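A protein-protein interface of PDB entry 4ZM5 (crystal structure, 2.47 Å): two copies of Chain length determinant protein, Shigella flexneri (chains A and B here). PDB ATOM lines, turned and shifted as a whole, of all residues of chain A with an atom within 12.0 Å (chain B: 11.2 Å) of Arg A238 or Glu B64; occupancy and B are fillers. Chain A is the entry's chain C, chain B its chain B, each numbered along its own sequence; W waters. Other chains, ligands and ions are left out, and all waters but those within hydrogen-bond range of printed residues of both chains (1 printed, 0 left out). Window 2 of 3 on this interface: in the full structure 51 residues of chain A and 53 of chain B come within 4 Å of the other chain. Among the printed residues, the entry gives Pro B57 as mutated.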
ATOM      1  N   GLU A   4      22.374 -10.408  -2.245  1.00  0.00           N
ATOM      2  CA  GLU A   4      22.382 -11.864  -2.471  1.00  0.00           C
ATOM      3  C   GLU A   4      23.503 -12.556  -1.642  1.00  0.00           C
ATOM      4  O   GLU A   4      24.666 -12.134  -1.705  1.00  0.00           O
ATOM      5  CB  GLU A   4      22.553 -12.164  -3.969  1.00  0.00           C
ATOM      6  CG  GLU A   4      22.119 -13.560  -4.368  1.00  0.00           C
ATOM      7  CD  GLU A   4      22.262 -13.868  -5.846  1.00  0.00           C
ATOM      8  OE1 GLU A   4      23.378 -13.688  -6.388  1.00  0.00           O
ATOM      9  OE2 GLU A   4      21.271 -14.337  -6.454  1.00  0.00           O
ATOM     10  N   LYS A   5      23.146 -13.622  -0.892  1.00  0.00           N
ATOM     11  CA  LYS A   5      24.072 -14.351  -0.016  1.00  0.00           C
ATOM     12  C   LYS A   5      24.064 -15.875  -0.246  1.00  0.00           C
ATOM     13  O   LYS A   5      23.040 -16.531  -0.037  1.00  0.00           O
ATOM     14  CB  LYS A   5      23.733 -14.074   1.465  1.00  0.00           C
ATOM     15  CG  LYS A   5      24.053 -12.672   1.968  1.00  0.00           C
ATOM     16  CD  LYS A   5      23.519 -12.474   3.386  1.00  0.00           C
ATOM     17  CE  LYS A   5      23.979 -11.180   4.014  1.00  0.00           C
ATOM     18  NZ  LYS A   5      23.307 -10.930   5.319  1.00  0.00           N
ATOM     19  N   TRP A   6      25.241 -16.434  -0.592  1.00  0.00           N
ATOM     20  CA  TRP A   6      25.512 -17.865  -0.791  1.00  0.00           C
ATOM     21  C   TRP A   6      26.524 -18.363   0.241  1.00  0.00           C
ATOM     22  O   TRP A   6      27.573 -17.739   0.401  1.00  0.00           O
ATOM     23  CB  TRP A   6      26.042 -18.147  -2.206  1.00  0.00           C
ATOM     24  CG  TRP A   6      25.109 -17.734  -3.303  1.00  0.00           C
ATOM     25  CD1 TRP A   6      24.886 -16.466  -3.753  1.00  0.00           C
ATOM     26  CD2 TRP A   6      24.323 -18.601  -4.138  1.00  0.00           C
ATOM     27  NE1 TRP A   6      24.000 -16.485  -4.804  1.00  0.00           N
ATOM     28  CE2 TRP A   6      23.632 -17.782  -5.058  1.00  0.00           C
ATOM     29  CE3 TRP A   6      24.123 -19.992  -4.189  1.00  0.00           C
ATOM     30  CZ2 TRP A   6      22.740 -18.305  -6.004  1.00  0.00           C
ATOM     31  CZ3 TRP A   6      23.263 -20.511  -5.144  1.00  0.00           C
ATOM     32  CH2 TRP A   6      22.560 -19.672  -6.018  1.00  0.00           C
ATOM     33  N   THR A   7      26.225 -19.490   0.922  1.00  0.00           N
ATOM     34  CA  THR A   7      27.103 -20.062   1.945  1.00  0.00           C
ATOM     35  C   THR A   7      27.801 -21.329   1.455  1.00  0.00           C
ATOM     36  O   THR A   7      27.150 -22.304   1.064  1.00  0.00           O
ATOM     37  CB  THR A   7      26.338 -20.327   3.267  1.00  0.00           C
ATOM     38  OG1 THR A   7      25.716 -19.114   3.688  1.00  0.00           O
ATOM     39  CG2 THR A   7      27.246 -20.833   4.398  1.00  0.00           C
ATOM     40  N   SER A   8      29.144 -21.308   1.510  1.00  0.00           N
ATOM     41  CA  SER A   8      29.985 -22.455   1.204  1.00  0.00           C
ATOM     42  C   SER A   8      30.438 -23.052   2.512  1.00  0.00           C
ATOM     43  O   SER A   8      30.829 -22.318   3.425  1.00  0.00           O
ATOM     44  CB  SER A   8      31.174 -22.052   0.345  1.00  0.00           C
ATOM     45  OG  SER A   8      31.959 -23.194   0.053  1.00  0.00           O
ATOM     46  N   THR A   9      30.374 -24.378   2.615  1.00  0.00           N
ATOM     47  CA  THR A   9      30.750 -25.083   3.833  1.00  0.00           C
ATOM     48  C   THR A   9      31.821 -26.143   3.552  1.00  0.00           C
ATOM     49  O   THR A   9      31.812 -26.802   2.515  1.00  0.00           O
ATOM     50  CB  THR A   9      29.481 -25.701   4.470  1.00  0.00           C
ATOM     51  OG1 THR A   9      28.537 -24.660   4.715  1.00  0.00           O
ATOM     52  CG2 THR A   9      29.757 -26.433   5.773  1.00  0.00           C
ATOM     53  N   SER A  85      32.659 -22.081   7.406  1.00  0.00           N
ATOM     54  CA  SER A  85      31.695 -21.512   6.480  1.00  0.00           C
ATOM     55  C   SER A  85      32.099 -20.133   6.017  1.00  0.00           C
ATOM     56  O   SER A  85      32.729 -19.380   6.758  1.00  0.00           O
ATOM     57  CB  SER A  85      30.307 -21.447   7.118  1.00  0.00           C
ATOM     58  OG  SER A  85      29.758 -22.749   7.244  1.00  0.00           O
ATOM     59  N   TYR A  86      31.710 -19.809   4.781  1.00  0.00           N
ATOM     60  CA  TYR A  86      31.909 -18.494   4.188  1.00  0.00           C
ATOM     61  C   TYR A  86      30.680 -18.060   3.414  1.00  0.00           C
ATOM     62  O   TYR A  86      30.140 -18.841   2.626  1.00  0.00           O
ATOM     63  CB  TYR A  86      33.143 -18.467   3.270  1.00  0.00           C
ATOM     64  CG  TYR A  86      33.407 -17.082   2.709  1.00  0.00           C
ATOM     65  CD1 TYR A  86      33.933 -16.072   3.512  1.00  0.00           C
ATOM     66  CD2 TYR A  86      33.077 -16.767   1.395  1.00  0.00           C
ATOM     67  CE1 TYR A  86      34.140 -14.785   3.014  1.00  0.00           C
ATOM     68  CE2 TYR A  86      33.274 -15.483   0.886  1.00  0.00           C
ATOM     69  CZ  TYR A  86      33.824 -14.500   1.694  1.00  0.00           C
ATOM     70  OH  TYR A  86      34.040 -13.241   1.190  1.00  0.00           O
ATOM     71  N   VAL A  87      30.265 -16.797   3.611  1.00  0.00           N
ATOM     72  CA  VAL A  87      29.138 -16.189   2.898  1.00  0.00           C
ATOM     73  C   VAL A  87      29.690 -15.295   1.776  1.00  0.00           C
ATOM     74  O   VAL A  87      30.327 -14.274   2.037  1.00  0.00           O
ATOM     75  CB  VAL A  87      28.119 -15.450   3.820  1.00  0.00           C
ATOM     76  CG1 VAL A  87      27.487 -16.429   4.808  1.00  0.00           C
ATOM     77  CG2 VAL A  87      28.742 -14.267   4.561  1.00  0.00           C
ATOM     78  N   GLY A  88      29.474 -15.722   0.538  1.00  0.00           N
ATOM     79  CA  GLY A  88      29.915 -14.990  -0.643  1.00  0.00           C
ATOM     80  C   GLY A  88      28.772 -14.366  -1.421  1.00  0.00           C
ATOM     81  O   GLY A  88      27.615 -14.439  -1.000  1.00  0.00           O
ATOM     82  N   GLN A  89      29.090 -13.751  -2.574  1.00  0.00           N
ATOM     83  CA  GLN A  89      28.102 -13.125  -3.457  1.00  0.00           C
ATOM     84  C   GLN A  89      27.546 -14.141  -4.465  1.00  0.00           C
ATOM     85  O   GLN A  89      26.413 -13.984  -4.935  1.00  0.00           O
ATOM     86  CB  GLN A  89      28.702 -11.918  -4.190  1.00  0.00           C
ATOM     87  CG  GLN A  89      28.765 -10.647  -3.349  1.00  0.00           C
ATOM     88  CD  GLN A  89      29.058  -9.427  -4.195  1.00  0.00           C
ATOM     89  OE1 GLN A  89      30.214  -9.049  -4.420  1.00  0.00           O
ATOM     90  NE2 GLN A  89      28.010  -8.790  -4.699  1.00  0.00           N
ATOM     91  N   THR A  90      28.339 -15.186  -4.777  1.00  0.00           N
ATOM     92  CA  THR A  90      27.944 -16.264  -5.682  1.00  0.00           C
ATOM     93  C   THR A  90      28.403 -17.598  -5.098  1.00  0.00           C
ATOM     94  O   THR A  90      29.211 -17.606  -4.177  1.00  0.00           O
ATOM     95  CB  THR A  90      28.436 -16.028  -7.124  1.00  0.00           C
ATOM     96  OG1 THR A  90      27.950 -17.090  -7.953  1.00  0.00           O
ATOM     97  CG2 THR A  90      29.971 -15.898  -7.241  1.00  0.00           C
ATOM     98  N   ALA A  91      27.861 -18.715  -5.614  1.00  0.00           N
ATOM     99  CA  ALA A  91      28.171 -20.075  -5.178  1.00  0.00           C
ATOM    100  C   ALA A  91      29.628 -20.430  -5.459  1.00  0.00           C
ATOM    101  O   ALA A  91      30.278 -21.057  -4.623  1.00  0.00           O
ATOM    102  CB  ALA A  91      27.254 -21.065  -5.879  1.00  0.00           C
ATOM    103  N   GLU A  92      30.134 -20.005  -6.637  1.00  0.00           N
ATOM    104  CA  GLU A  92      31.490 -20.244  -7.126  1.00  0.00           C
ATOM    105  C   GLU A  92      32.514 -19.407  -6.348  1.00  0.00           C
ATOM    106  O   GLU A  92      33.580 -19.929  -5.995  1.00  0.00           O
ATOM    107  CB  GLU A  92      31.574 -19.950  -8.638  1.00  0.00           C
ATOM    108  CG  GLU A  92      30.931 -21.012  -9.525  1.00  0.00           C
ATOM    109  CD  GLU A  92      29.422 -20.990  -9.734  1.00  0.00           C
ATOM    110  OE1 GLU A  92      28.957 -21.702 -10.652  1.00  0.00           O
ATOM    111  OE2 GLU A  92      28.702 -20.287  -8.984  1.00  0.00           O
ATOM    112  N   GLY A  93      32.178 -18.133  -6.098  1.00  0.00           N
ATOM    113  CA  GLY A  93      32.999 -17.190  -5.344  1.00  0.00           C
ATOM    114  C   GLY A  93      33.113 -17.553  -3.874  1.00  0.00           C
ATOM    115  O   GLY A  93      34.217 -17.535  -3.320  1.00  0.00           O
ATOM    116  N   ALA A  94      31.973 -17.915  -3.237  1.00  0.00           N
ATOM    117  CA  ALA A  94      31.936 -18.324  -1.836  1.00  0.00           C
ATOM    118  C   ALA A  94      32.795 -19.575  -1.623  1.00  0.00           C
ATOM    119  O   ALA A  94      33.526 -19.641  -0.637  1.00  0.00           O
ATOM    120  CB  ALA A  94      30.500 -18.586  -1.393  1.00  0.00           C
ATOM    121  N   GLN A  95      32.704 -20.557  -2.546  1.00  0.00           N
ATOM    122  CA  GLN A  95      33.471 -21.800  -2.497  1.00  0.00           C
ATOM    123  C   GLN A  95      34.972 -21.499  -2.642  1.00  0.00           C
ATOM    124  O   GLN A  95      35.779 -21.959  -1.835  1.00  0.00           O
ATOM    125  CB  GLN A  95      32.969 -22.776  -3.581  1.00  0.00           C
ATOM    126  CG  GLN A  95      33.735 -24.089  -3.624  1.00  0.00           C
ATOM    127  CD  GLN A  95      33.330 -24.908  -4.812  1.00  0.00           C
ATOM    128  OE1 GLN A  95      33.510 -24.509  -5.968  1.00  0.00           O
ATOM    129  NE2 GLN A  95      32.808 -26.088  -4.560  1.00  0.00           N
ATOM    130  N   THR A 234      31.912 -26.741  -0.254  1.00  0.00           N
ATOM    131  CA  THR A 234      30.769 -27.051  -1.114  1.00  0.00           C
ATOM    132  C   THR A 234      30.473 -25.932  -2.066  1.00  0.00           C
ATOM    133  O   THR A 234      30.847 -24.781  -1.820  1.00  0.00           O
ATOM    134  CB  THR A 234      29.485 -27.330  -0.286  1.00  0.00           C
ATOM    135  OG1 THR A 234      29.106 -26.169   0.471  1.00  0.00           O
ATOM    136  CG2 THR A 234      29.581 -28.585   0.566  1.00  0.00           C
ATOM    137  N   LEU A 235      29.760 -26.279  -3.138  1.00  0.00           N
ATOM    138  CA  LEU A 235      29.198 -25.351  -4.103  1.00  0.00           C
ATOM    139  C   LEU A 235      27.695 -25.278  -3.763  1.00  0.00           C
ATOM    140  O   LEU A 235      26.959 -26.242  -4.042  1.00  0.00           O
ATOM    141  CB  LEU A 235      29.465 -25.811  -5.544  1.00  0.00           C
ATOM    142  CG  LEU A 235      29.014 -24.862  -6.651  1.00  0.00           C
ATOM    143  CD1 LEU A 235      29.933 -23.662  -6.746  1.00  0.00           C
ATOM    144  CD2 LEU A 235      28.988 -25.577  -7.969  1.00  0.00           C
ATOM    145  N   PRO A 236      27.246 -24.212  -3.054  1.00  0.00           N
ATOM    146  CA  PRO A 236      25.823 -24.139  -2.652  1.00  0.00           C
ATOM    147  C   PRO A 236      24.851 -24.179  -3.835  1.00  0.00           C
ATOM    148  O   PRO A 236      25.055 -23.502  -4.842  1.00  0.00           O
ATOM    149  CB  PRO A 236      25.722 -22.811  -1.892  1.00  0.00           C
ATOM    150  CG  PRO A 236      26.929 -22.039  -2.272  1.00  0.00           C
ATOM    151  CD  PRO A 236      28.002 -23.023  -2.605  1.00  0.00           C
ATOM    152  N   ILE A 237      23.814 -25.019  -3.709  1.00  0.00           N
ATOM    153  CA  ILE A 237      22.801 -25.241  -4.731  1.00  0.00           C
ATOM    154  C   ILE A 237      21.781 -24.077  -4.731  1.00  0.00           C
ATOM    155  O   ILE A 237      21.176 -23.787  -5.767  1.00  0.00           O
ATOM    156  CB  ILE A 237      22.150 -26.643  -4.554  1.00  0.00           C
ATOM    157  CG1 ILE A 237      21.638 -27.207  -5.893  1.00  0.00           C
ATOM    158  CG2 ILE A 237      21.093 -26.687  -3.446  1.00  0.00           C
ATOM    159  CD1 ILE A 237      21.452 -28.742  -5.937  1.00  0.00           C
ATOM    160  N   ARG A 238      21.627 -23.391  -3.586  1.00  0.00           N
ATOM    161  CA  ARG A 238      20.710 -22.260  -3.445  1.00  0.00           C
ATOM    162  C   ARG A 238      21.262 -21.237  -2.442  1.00  0.00           C
ATOM    163  O   ARG A 238      22.169 -21.561  -1.673  1.00  0.00           O
ATOM    164  CB  ARG A 238      19.307 -22.746  -3.025  1.00  0.00           C
ATOM    165  CG  ARG A 238      19.209 -23.264  -1.589  1.00  0.00           C
ATOM    166  CD  ARG A 238      17.908 -23.984  -1.314  1.00  0.00           C
ATOM    167  NE  ARG A 238      18.105 -25.431  -1.363  1.00  0.00           N
ATOM    168  CZ  ARG A 238      17.641 -26.228  -2.319  1.00  0.00           C
ATOM    169  NH1 ARG A 238      16.901 -25.737  -3.301  1.00  0.00           N
ATOM    170  NH2 ARG A 238      17.879 -27.529  -2.278  1.00  0.00           N
ATOM    171  N   ARG A 239      20.698 -20.025  -2.434  1.00  0.00           N
ATOM    172  CA  ARG A 239      21.123 -18.975  -1.522  1.00  0.00           C
ATOM    173  C   ARG A 239      20.397 -19.106  -0.180  1.00  0.00           C
ATOM    174  O   ARG A 239      19.369 -19.781  -0.104  1.00  0.00           O
ATOM    175  CB  ARG A 239      20.896 -17.591  -2.154  1.00  0.00           C
ATOM    176  CG  ARG A 239      19.459 -17.089  -2.168  1.00  0.00           C
ATOM    177  CD  ARG A 239      19.386 -15.700  -2.761  1.00  0.00           C
ATOM    178  NE  ARG A 239      19.579 -15.724  -4.213  1.00  0.00           N
ATOM    179  CZ  ARG A 239      18.594 -15.681  -5.106  1.00  0.00           C
ATOM    180  NH1 ARG A 239      17.330 -15.602  -4.706  1.00  0.00           N
ATOM    181  NH2 ARG A 239      18.865 -15.716  -6.403  1.00  0.00           N
ATOM    182  N   ASP A 240      20.918 -18.449   0.870  1.00  0.00           N
ATOM    183  CA  ASP A 240      20.315 -18.454   2.210  1.00  0.00           C
ATOM    184  C   ASP A 240      19.102 -17.518   2.258  1.00  0.00           C
ATOM    185  O   ASP A 240      18.169 -17.738   3.031  1.00  0.00           O
ATOM    186  CB  ASP A 240      21.353 -18.043   3.270  1.00  0.00           C
ATOM    187  CG  ASP A 240      22.798 -18.285   2.867  1.00  0.00           C
ATOM    188  OD1 ASP A 240      23.141 -19.448   2.538  1.00  0.00           O
ATOM    189  OD2 ASP A 240      23.578 -17.313   2.857  1.00  0.00           O
ATOM    190  N   PRO B  57      25.095 -34.933   6.785  1.00  0.00           N
ATOM    191  CA  PRO B  57      24.039 -33.941   7.027  1.00  0.00           C
ATOM    192  C   PRO B  57      24.144 -32.730   6.101  1.00  0.00           C
ATOM    193  O   PRO B  57      23.128 -32.295   5.572  1.00  0.00           O
ATOM    194  CB  PRO B  57      24.263 -33.548   8.490  1.00  0.00           C
ATOM    195  CG  PRO B  57      24.842 -34.750   9.112  1.00  0.00           C
ATOM    196  CD  PRO B  57      25.756 -35.295   8.061  1.00  0.00           C
ATOM    197  N   GLU B  58      25.371 -32.244   5.856  1.00  0.00           N
ATOM    198  CA  GLU B  58      25.666 -31.103   4.982  1.00  0.00           C
ATOM    199  C   GLU B  58      25.423 -31.407   3.508  1.00  0.00           C
ATOM    200  O   GLU B  58      24.817 -30.579   2.819  1.00  0.00           O
ATOM    201  CB  GLU B  58      27.118 -30.638   5.160  1.00  0.00           C
ATOM    202  CG  GLU B  58      27.411 -30.041   6.530  1.00  0.00           C
ATOM    203  CD  GLU B  58      26.836 -28.670   6.841  1.00  0.00           C
ATOM    204  OE1 GLU B  58      26.287 -28.004   5.933  1.00  0.00           O
ATOM    205  OE2 GLU B  58      26.980 -28.244   8.006  1.00  0.00           O
ATOM    206  N   THR B  59      25.932 -32.557   3.016  1.00  0.00           N
ATOM    207  CA  THR B  59      25.816 -32.988   1.617  1.00  0.00           C
ATOM    208  C   THR B  59      24.348 -33.310   1.249  1.00  0.00           C
ATOM    209  O   THR B  59      23.886 -32.939   0.169  1.00  0.00           O
ATOM    210  CB  THR B  59      26.755 -34.179   1.401  1.00  0.00           C
ATOM    211  OG1 THR B  59      28.093 -33.715   1.479  1.00  0.00           O
ATOM    212  CG2 THR B  59      26.535 -34.900   0.097  1.00  0.00           C
ATOM    213  N   LEU B  60      23.631 -34.000   2.140  1.00  0.00           N
ATOM    214  CA  LEU B  60      22.234 -34.382   1.914  1.00  0.00           C
ATOM    215  C   LEU B  60      21.300 -33.163   1.871  1.00  0.00           C
ATOM    216  O   LEU B  60      20.278 -33.208   1.186  1.00  0.00           O
ATOM    217  CB  LEU B  60      21.758 -35.398   2.971  1.00  0.00           C
ATOM    218  CG  LEU B  60      22.354 -36.811   2.868  1.00  0.00           C
ATOM    219  CD1 LEU B  60      21.751 -37.719   3.898  1.00  0.00           C
ATOM    220  CD2 LEU B  60      22.096 -37.413   1.510  1.00  0.00           C
ATOM    221  N   ASP B  61      21.667 -32.077   2.557  1.00  0.00           N
ATOM    222  CA  ASP B  61      20.917 -30.827   2.570  1.00  0.00           C
ATOM    223  C   ASP B  61      21.169 -30.018   1.281  1.00  0.00           C
ATOM    224  O   ASP B  61      20.251 -29.360   0.772  1.00  0.00           O
ATOM    225  CB  ASP B  61      21.311 -29.994   3.794  1.00  0.00           C
ATOM    226  CG  ASP B  61      20.464 -28.760   3.987  1.00  0.00           C
ATOM    227  OD1 ASP B  61      19.297 -28.904   4.432  1.00  0.00           O
ATOM    228  OD2 ASP B  61      20.954 -27.645   3.669  1.00  0.00           O
ATOM    229  N   ASN B  62      22.413 -30.069   0.759  1.00  0.00           N
ATOM    230  CA  ASN B  62      22.814 -29.340  -0.441  1.00  0.00           C
ATOM    231  C   ASN B  62      22.518 -30.156  -1.718  1.00  0.00           C
ATOM    232  O   ASN B  62      23.378 -30.334  -2.583  1.00  0.00           O
ATOM    233  CB  ASN B  62      24.286 -28.933  -0.363  1.00  0.00           C
ATOM    234  CG  ASN B  62      24.641 -27.851  -1.344  1.00  0.00           C
ATOM    235  OD1 ASN B  62      24.005 -26.798  -1.401  1.00  0.00           O
ATOM    236  ND2 ASN B  62      25.635 -28.105  -2.166  1.00  0.00           N
ATOM    237  N   GLN B  63      21.263 -30.606  -1.831  1.00  0.00           N
ATOM    238  CA  GLN B  63      20.713 -31.373  -2.948  1.00  0.00           C
ATOM    239  C   GLN B  63      19.502 -30.658  -3.523  1.00  0.00           C
ATOM    240  O   GLN B  63      18.943 -29.812  -2.824  1.00  0.00           O
ATOM    241  CB  GLN B  63      20.270 -32.753  -2.450  1.00  0.00           C
ATOM    242  CG  GLN B  63      21.379 -33.729  -2.123  1.00  0.00           C
ATOM    243  CD  GLN B  63      20.790 -35.071  -1.762  1.00  0.00           C
ATOM    244  OE1 GLN B  63      21.393 -36.121  -1.999  1.00  0.00           O
ATOM    245  NE2 GLN B  63      19.595 -35.069  -1.158  1.00  0.00           N
ATOM    246  N   GLU B  64      19.050 -31.033  -4.760  1.00  0.00           N
ATOM    247  CA  GLU B  64      17.832 -30.492  -5.388  1.00  0.00           C
ATOM    248  C   GLU B  64      16.653 -30.682  -4.415  1.00  0.00           C
ATOM    249  O   GLU B  64      15.976 -29.712  -4.055  1.00  0.00           O
ATOM    250  CB  GLU B  64      17.554 -31.185  -6.737  1.00  0.00           C
ATOM    251  CG  GLU B  64      17.994 -30.395  -7.957  1.00  0.00           C
ATOM    252  CD  GLU B  64      17.613 -31.007  -9.295  1.00  0.00           C
ATOM    253  OE1 GLU B  64      18.529 -31.299 -10.099  1.00  0.00           O
ATOM    254  OE2 GLU B  64      16.399 -31.181  -9.547  1.00  0.00           O
ATOM    255  N   GLU B  65      16.477 -31.937  -3.938  1.00  0.00           N
ATOM    256  CA  GLU B  65      15.494 -32.336  -2.934  1.00  0.00           C
ATOM    257  C   GLU B  65      16.289 -32.642  -1.656  1.00  0.00           C
ATOM    258  O   GLU B  65      16.964 -33.678  -1.560  1.00  0.00           O
ATOM    259  CB  GLU B  65      14.630 -33.522  -3.418  1.00  0.00           C
ATOM    260  CG  GLU B  65      13.285 -33.666  -2.707  1.00  0.00           C
ATOM    261  CD  GLU B  65      13.281 -34.232  -1.293  1.00  0.00           C
ATOM    262  OE1 GLU B  65      14.210 -34.998  -0.941  1.00  0.00           O
ATOM    263  OE2 GLU B  65      12.323 -33.930  -0.543  1.00  0.00           O
ATOM    264  N   PRO B  66      16.305 -31.682  -0.709  1.00  0.00           N
ATOM    265  CA  PRO B  66      17.095 -31.868   0.515  1.00  0.00           C
ATOM    266  C   PRO B  66      16.614 -33.006   1.417  1.00  0.00           C
ATOM    267  O   PRO B  66      15.408 -33.188   1.628  1.00  0.00           O
ATOM    268  CB  PRO B  66      16.951 -30.528   1.245  1.00  0.00           C
ATOM    269  CG  PRO B  66      16.362 -29.589   0.283  1.00  0.00           C
ATOM    270  CD  PRO B  66      15.594 -30.388  -0.699  1.00  0.00           C
ATOM    271  N   GLU B  67      17.581 -33.750   1.969  1.00  0.00           N
ATOM    272  CA  GLU B  67      17.319 -34.841   2.898  1.00  0.00           C
ATOM    273  C   GLU B  67      17.784 -34.405   4.284  1.00  0.00           C
ATOM    274  O   GLU B  67      18.745 -33.632   4.415  1.00  0.00           O
ATOM    275  CB  GLU B  67      18.009 -36.146   2.452  1.00  0.00           C
ATOM    276  CG  GLU B  67      17.408 -36.801   1.213  1.00  0.00           C
ATOM    277  CD  GLU B  67      18.204 -37.963   0.628  1.00  0.00           C
ATOM    278  OE1 GLU B  67      18.686 -37.829  -0.521  1.00  0.00           O
ATOM    279  OE2 GLU B  67      18.337 -39.012   1.302  1.00  0.00           O
ATOM    280  N   LYS B  68      17.074 -34.867   5.314  1.00  0.00           N
ATOM    281  CA  LYS B  68      17.402 -34.546   6.689  1.00  0.00           C
ATOM    282  C   LYS B  68      18.020 -35.767   7.359  1.00  0.00           C
ATOM    283  O   LYS B  68      17.358 -36.792   7.559  1.00  0.00           O
ATOM    284  CB  LYS B  68      16.156 -34.027   7.457  1.00  0.00           C
ATOM    285  CG  LYS B  68      16.325 -33.844   8.972  1.00  0.00           C
ATOM    286  CD  LYS B  68      17.091 -32.580   9.357  1.00  0.00           C
ATOM    287  CE  LYS B  68      16.733 -32.126  10.757  1.00  0.00           C
ATOM    288  NZ  LYS B  68      17.570 -30.973  11.197  1.00  0.00           N
HETATM  289  O   HOH W   1      19.973 -26.156   0.366  1.00  0.00           O
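Water W1 lies within hydrogen-bond range of NE of Arg A238 (2.6 Å) and O of Asp B61 (3.2 Å).
The backbone carbonyl oxygen (O) of Leu B60 is in hydrogen-bond range of the side-chain amide nitrogen (NE2) of Gln B63 (3.1 Å). NE2 of Gln B63 sits at hydrogen-bond distance from O of Glu B65, at 3.0 Å. The side-chain carboxylate (OE1) of Glu B67 is in hydrogen-bond range of the side-chain amide nitrogen (NE2) of Gln B63 (3.0 Å). The side-chain hydroxyl of Ser A85 is in hydrogen-bond range of the side-chain hydroxyl of Thr A9, 3.4 Å away. O of Thr A9 is in hydrogen-bond range of N of Thr A234. The side-chain amide nitrogen (NE2) of Gln A95 sits close to the backbone NH (N) of Leu A235, at 3.4 Å.
Among the printed residues, merely in contact across the chains: Thr A9 with Glu B58, Pro A236 with Asn B62, Ile A237 with Gln B63, Ile A237 with Glu B64 and Arg A238 with Pro B66.
Printed residues of chain B within 4 Å of Thr A9: Glu B58 (3.8 Å). Thr A90 touches none of the printed residues of chain B. Printed residues of chain B within 4 Å of Leu A235: Asn B62. Of chain B, only Asn B62 comes within 4 Å of Pro A236. Ile A237 touches just these residues of chain B: Asn B62 (2.9 Å), Gln B63 (3.6 Å) and Glu B64 (3.5 Å). Printed residues of chain B within 4 Å of Arg A238: Gln B63, Glu B64 and Pro B66. Printed residues of chain A within 4 Å of Glu B58: Thr A9 (3.8 Å). No residue of chain A comes within 4 Å of Asp B61. Asn B62 touches just these residues of chain A: Leu A235, Pro A236 and Ile A237. Of chain A, only Ile A237 (3.6 Å) and Arg A238 (2.6 Å) come within 4 Å of Gln B63. Of chain A, only Ile A237 (3.5 Å) and Arg A238 (3.4 Å) come within 4 Å of Glu B64. No residue of chain A comes within 4 Å of Glu B65. Of chain A, only Arg A238 (3.6 Å) comes within 4 Å of Pro B66. The nearest residue of chain B that does not touch Arg A238 is Asp B61 (4.3 Å). The nearest residue of chain A that does not touch Glu B64 is Pro A236 (9.0 Å). The nearest printed residue of chain B that does not touch Thr A9 is Asn B62 (7.7 Å).
No position is printed for both chains. Of the 9 pairs that touch across the chains among the printed residues, none has its exchanged pair printed and touching as well.
Of the 12 printed residues of chain B, 5 touch a printed residue of chain A. Hydrophobic or aromatic side chains of chain B within 4 Å of the printed part of chain A: Pro B66. Of the 24 printed residues of chain A, 5 touch a printed residue of chain B. Along chain A the printed residues that touch a printed residue of chain B span positions 9 to 238.
The backbone carbonyl oxygen (O) of Leu A235 lies within hydrogen-bond range of the side-chain amide nitrogen (ND2) of Asn B62. OD1 of Asn B62 sits at hydrogen-bond distance from N of Ile A237, 2.9 Å away. The backbone carbonyl oxygen of Gln B63 is in hydrogen-bond range of the guanidinium group of Arg A238. The backbone carbonyl oxygen of Glu B64 lies within hydrogen-bond range of the guanidinium group of Arg A238 (3.4 Å).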
